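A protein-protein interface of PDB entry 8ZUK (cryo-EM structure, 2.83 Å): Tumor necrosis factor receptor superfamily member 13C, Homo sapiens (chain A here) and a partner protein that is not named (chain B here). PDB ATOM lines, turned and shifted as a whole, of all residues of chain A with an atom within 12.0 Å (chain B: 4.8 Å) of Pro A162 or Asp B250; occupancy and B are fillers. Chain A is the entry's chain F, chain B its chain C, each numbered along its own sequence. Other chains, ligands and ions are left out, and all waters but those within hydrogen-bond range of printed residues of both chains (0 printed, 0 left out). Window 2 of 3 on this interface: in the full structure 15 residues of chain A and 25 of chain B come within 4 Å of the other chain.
The side-chain carboxylate (OD2) of Asp B250 sits at hydrogen-bond distance from the side-chain hydroxyl (OG) of Ser B253 (2.9 Å). The side-chain carboxylate of Asp B250 lies close to the side-chain amide oxygen of Asn B252.
Printed residues of chain B within 4 Å of Ser A160: Phe B247. Pro A162 touches four residues of chain B. Printed residues of chain B within 4 Å of Val A163: Ser B267 and Gly B268. Of chain A, only Ser A160 (3.3 Å) and Pro A162 (3.5 Å) come within 4 Å of Phe B247. Printed residues of chain A within 4 Å of Lys B248: Pro A162 (3.6 Å). No residue of chain A comes within 4 Å of Pro B249. No residue of chain A comes within 4 Å of Pro B251. No residue of chain A comes within 4 Å of Ser B253. Ser B267 touches just these residues of chain A: Pro A162 (3.3 Å) and Val A163 (3.5 Å). The nearest residue of chain A that does not touch Asp B250 is Val A161 (5.8 Å).
The backbone NH (N) of Gly B268 sits at hydrogen-bond distance from the backbone carbonyl oxygen (O) of Val A163 (3.1 Å).
Phe B247 touches Ser A160 (CB to O, 3.3 Å). CD2 of Phe B247 touches CG of Pro A162, at 3.5 Å. O of Lys B248 touches CG of Pro A162, at 3.6 Å. Pro A162 touches Asp B250. Pro A162 touches Ser B267. Ser B267 touches Val A163 (CA to O, 3.5 Å).
Of the 7 printed residues of chain A, 3 touch a printed residue of chain B. Of the 10 printed residues of chain B, 5 touch a printed residue of chain A. Printed residues of chain B that touch a printed residue of chain A: Phe B247, Lys B248, Asp B250, Ser B267 and Gly B268. Hydrophobic or aromatic side chains of chain B that line the printed part of chain A: Phe B247. Among the printed residues, no Asp or Glu carboxylate lies within 4 Å of a Lys or Arg side-chain nitrogen of the other chain.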
ATOM      1  N   SER A 160      28.011 -16.628 -26.982  1.00  0.00           N
ATOM      2  CA  SER A 160      27.247 -15.720 -27.828  1.00  0.00           C
ATOM      3  C   SER A 160      25.750 -15.968 -27.686  1.00  0.00           C
ATOM      4  O   SER A 160      24.932 -15.191 -28.177  1.00  0.00           O
ATOM      5  CB  SER A 160      27.668 -15.867 -29.291  1.00  0.00           C
ATOM      6  OG  SER A 160      26.900 -15.022 -30.131  1.00  0.00           O
ATOM      7  N   VAL A 161      25.397 -17.058 -27.010  1.00  0.00           N
ATOM      8  CA  VAL A 161      23.999 -17.421 -26.800  1.00  0.00           C
ATOM      9  C   VAL A 161      23.390 -16.466 -25.780  1.00  0.00           C
ATOM     10  O   VAL A 161      23.923 -16.325 -24.669  1.00  0.00           O
ATOM     11  CB  VAL A 161      23.863 -18.881 -26.343  1.00  0.00           C
ATOM     12  CG1 VAL A 161      22.435 -19.168 -25.899  1.00  0.00           C
ATOM     13  CG2 VAL A 161      24.280 -19.825 -27.459  1.00  0.00           C
ATOM     14  N   PRO A 162      22.296 -15.784 -26.113  1.00  0.00           N
ATOM     15  CA  PRO A 162      21.653 -14.897 -25.136  1.00  0.00           C
ATOM     16  C   PRO A 162      21.166 -15.672 -23.920  1.00  0.00           C
ATOM     17  O   PRO A 162      20.726 -16.820 -24.025  1.00  0.00           O
ATOM     18  CB  PRO A 162      20.485 -14.291 -25.922  1.00  0.00           C
ATOM     19  CG  PRO A 162      20.885 -14.428 -27.358  1.00  0.00           C
ATOM     20  CD  PRO A 162      21.642 -15.720 -27.429  1.00  0.00           C
ATOM     21  N   VAL A 163      21.247 -15.032 -22.759  1.00  0.00           N
ATOM     22  CA  VAL A 163      20.832 -15.619 -21.493  1.00  0.00           C
ATOM     23  C   VAL A 163      19.711 -14.760 -20.919  1.00  0.00           C
ATOM     24  O   VAL A 163      19.879 -13.546 -20.775  1.00  0.00           O
ATOM     25  CB  VAL A 163      21.996 -15.730 -20.495  1.00  0.00           C
ATOM     26  CG1 VAL A 163      21.562 -16.506 -19.262  1.00  0.00           C
ATOM     27  CG2 VAL A 163      23.197 -16.392 -21.151  1.00  0.00           C
ATOM     28  N   PRO A 164      18.555 -15.335 -20.584  1.00  0.00           N
ATOM     29  CA  PRO A 164      17.465 -14.531 -20.014  1.00  0.00           C
ATOM     30  C   PRO A 164      17.808 -13.967 -18.646  1.00  0.00           C
ATOM     31  O   PRO A 164      18.833 -14.324 -18.056  1.00  0.00           O
ATOM     32  CB  PRO A 164      16.302 -15.529 -19.932  1.00  0.00           C
ATOM     33  CG  PRO A 164      16.642 -16.585 -20.941  1.00  0.00           C
ATOM     34  CD  PRO A 164      18.130 -16.718 -20.847  1.00  0.00           C
ATOM     35  N   ALA A 165      16.955 -13.089 -18.130  1.00  0.00           N
ATOM     36  CA  ALA A 165      17.170 -12.458 -16.841  1.00  0.00           C
ATOM     37  C   ALA A 165      16.442 -13.229 -15.744  1.00  0.00           C
ATOM     38  O   ALA A 165      15.773 -14.237 -15.987  1.00  0.00           O
ATOM     39  CB  ALA A 165      16.719 -10.998 -16.877  1.00  0.00           C
ATOM     40  N   THR A 166      16.577 -12.739 -14.516  1.00  0.00           N
ATOM     41  CA  THR A 166      15.970 -13.326 -13.327  1.00  0.00           C
ATOM     42  C   THR A 166      15.176 -12.264 -12.577  1.00  0.00           C
ATOM     43  O   THR A 166      15.365 -12.032 -11.381  1.00  0.00           O
ATOM     44  CB  THR A 166      17.029 -13.965 -12.431  1.00  0.00           C
ATOM     45  OG1 THR A 166      17.977 -14.667 -13.244  1.00  0.00           O
ATOM     46  CG2 THR A 166      16.389 -14.960 -11.470  1.00  0.00           C
ATOM     47  N   PHE B 247      26.782 -10.344 -29.480  1.00  0.00           N
ATOM     48  CA  PHE B 247      25.911 -11.498 -29.632  1.00  0.00           C
ATOM     49  C   PHE B 247      24.830 -11.178 -30.653  1.00  0.00           C
ATOM     50  O   PHE B 247      24.569 -10.016 -30.972  1.00  0.00           O
ATOM     51  CB  PHE B 247      25.290 -11.910 -28.291  1.00  0.00           C
ATOM     52  CG  PHE B 247      24.059 -11.131 -27.923  1.00  0.00           C
ATOM     53  CD1 PHE B 247      24.165  -9.883 -27.336  1.00  0.00           C
ATOM     54  CD2 PHE B 247      22.795 -11.653 -28.152  1.00  0.00           C
ATOM     55  CE1 PHE B 247      23.035  -9.164 -26.993  1.00  0.00           C
ATOM     56  CE2 PHE B 247      21.662 -10.938 -27.813  1.00  0.00           C
ATOM     57  CZ  PHE B 247      21.782  -9.693 -27.233  1.00  0.00           C
ATOM     58  N   LYS B 248      24.202 -12.235 -31.165  1.00  0.00           N
ATOM     59  CA  LYS B 248      23.108 -12.127 -32.120  1.00  0.00           C
ATOM     60  C   LYS B 248      21.795 -12.456 -31.425  1.00  0.00           C
ATOM     61  O   LYS B 248      21.720 -13.471 -30.715  1.00  0.00           O
ATOM     62  CB  LYS B 248      23.331 -13.070 -33.304  1.00  0.00           C
ATOM     63  CG  LYS B 248      22.107 -13.286 -34.186  1.00  0.00           C
ATOM     64  CD  LYS B 248      21.763 -12.050 -35.011  1.00  0.00           C
ATOM     65  CE  LYS B 248      23.001 -11.412 -35.626  1.00  0.00           C
ATOM     66  NZ  LYS B 248      22.645 -10.351 -36.610  1.00  0.00           N
ATOM     67  N   PRO B 249      20.760 -11.629 -31.577  1.00  0.00           N
ATOM     68  CA  PRO B 249      19.484 -11.907 -30.906  1.00  0.00           C
ATOM     69  C   PRO B 249      18.923 -13.277 -31.263  1.00  0.00           C
ATOM     70  O   PRO B 249      18.996 -13.724 -32.411  1.00  0.00           O
ATOM     71  CB  PRO B 249      18.574 -10.786 -31.416  1.00  0.00           C
ATOM     72  CG  PRO B 249      19.500  -9.650 -31.657  1.00  0.00           C
ATOM     73  CD  PRO B 249      20.819 -10.250 -32.094  1.00  0.00           C
ATOM     74  N   ASP B 250      18.363 -13.939 -30.260  1.00  0.00           N
ATOM     75  CA  ASP B 250      17.771 -15.258 -30.443  1.00  0.00           C
ATOM     76  C   ASP B 250      16.482 -15.129 -31.247  1.00  0.00           C
ATOM     77  O   ASP B 250      15.588 -14.369 -30.851  1.00  0.00           O
ATOM     78  CB  ASP B 250      17.502 -15.895 -29.081  1.00  0.00           C
ATOM     79  CG  ASP B 250      17.178 -17.376 -29.170  1.00  0.00           C
ATOM     80  OD1 ASP B 250      16.869 -17.870 -30.273  1.00  0.00           O
ATOM     81  OD2 ASP B 250      17.233 -18.053 -28.122  1.00  0.00           O
ATOM     82  N   PRO B 251      16.345 -15.834 -32.373  1.00  0.00           N
ATOM     83  CA  PRO B 251      15.150 -15.664 -33.216  1.00  0.00           C
ATOM     84  C   PRO B 251      13.840 -16.054 -32.547  1.00  0.00           C
ATOM     85  O   PRO B 251      12.774 -15.622 -32.999  1.00  0.00           O
ATOM     86  CB  PRO B 251      15.442 -16.572 -34.418  1.00  0.00           C
ATOM     87  CG  PRO B 251      16.923 -16.669 -34.473  1.00  0.00           C
ATOM     88  CD  PRO B 251      17.404 -16.602 -33.054  1.00  0.00           C
ATOM     89  N   ASN B 252      13.880 -16.858 -31.481  1.00  0.00           N
ATOM     90  CA  ASN B 252      12.648 -17.349 -30.869  1.00  0.00           C
ATOM     91  C   ASN B 252      12.634 -17.125 -29.359  1.00  0.00           C
ATOM     92  O   ASN B 252      12.255 -18.024 -28.600  1.00  0.00           O
ATOM     93  CB  ASN B 252      12.437 -18.829 -31.209  1.00  0.00           C
ATOM     94  CG  ASN B 252      13.569 -19.718 -30.718  1.00  0.00           C
ATOM     95  OD1 ASN B 252      14.482 -19.268 -30.028  1.00  0.00           O
ATOM     96  ND2 ASN B 252      13.510 -20.995 -31.079  1.00  0.00           N
ATOM     97  N   SER B 253      13.032 -15.935 -28.917  1.00  0.00           N
ATOM     98  CA  SER B 253      12.997 -15.574 -27.507  1.00  0.00           C
ATOM     99  C   SER B 253      11.990 -14.453 -27.289  1.00  0.00           C
ATOM    100  O   SER B 253      11.783 -13.614 -28.173  1.00  0.00           O
ATOM    101  CB  SER B 253      14.379 -15.146 -27.007  1.00  0.00           C
ATOM    102  OG  SER B 253      15.251 -16.260 -26.920  1.00  0.00           O
ATOM    103  N   PHE B 256      13.054 -10.619 -27.884  1.00  0.00           N
ATOM    104  CA  PHE B 256      13.164  -9.965 -29.179  1.00  0.00           C
ATOM    105  C   PHE B 256      11.889 -10.052 -30.008  1.00  0.00           C
ATOM    106  O   PHE B 256      11.925  -9.765 -31.209  1.00  0.00           O
ATOM    107  CB  PHE B 256      14.339 -10.554 -29.967  1.00  0.00           C
ATOM    108  CG  PHE B 256      15.580 -10.745 -29.145  1.00  0.00           C
ATOM    109  CD1 PHE B 256      16.393  -9.668 -28.835  1.00  0.00           C
ATOM    110  CD2 PHE B 256      15.930 -11.999 -28.673  1.00  0.00           C
ATOM    111  CE1 PHE B 256      17.534  -9.837 -28.074  1.00  0.00           C
ATOM    112  CE2 PHE B 256      17.069 -12.176 -27.911  1.00  0.00           C
ATOM    113  CZ  PHE B 256      17.872 -11.094 -27.612  1.00  0.00           C
ATOM    114  N   SER B 267      17.624  -9.558 -21.560  1.00  0.00           N
ATOM    115  CA  SER B 267      18.507 -10.596 -22.071  1.00  0.00           C
ATOM    116  C   SER B 267      19.916 -10.040 -22.204  1.00  0.00           C
ATOM    117  O   SER B 267      20.101  -8.897 -22.627  1.00  0.00           O
ATOM    118  CB  SER B 267      18.023 -11.124 -23.427  1.00  0.00           C
ATOM    119  OG  SER B 267      18.925 -12.081 -23.950  1.00  0.00           O
ATOM    120  N   GLY B 268      20.905 -10.854 -21.845  1.00  0.00           N
ATOM    121  CA  GLY B 268      22.287 -10.424 -21.924  1.00  0.00           C
ATOM    122  C   GLY B 268      23.272 -11.436 -21.379  1.00  0.00           C
ATOM    123  O   GLY B 268      23.049 -12.646 -21.475  1.00  0.00           O
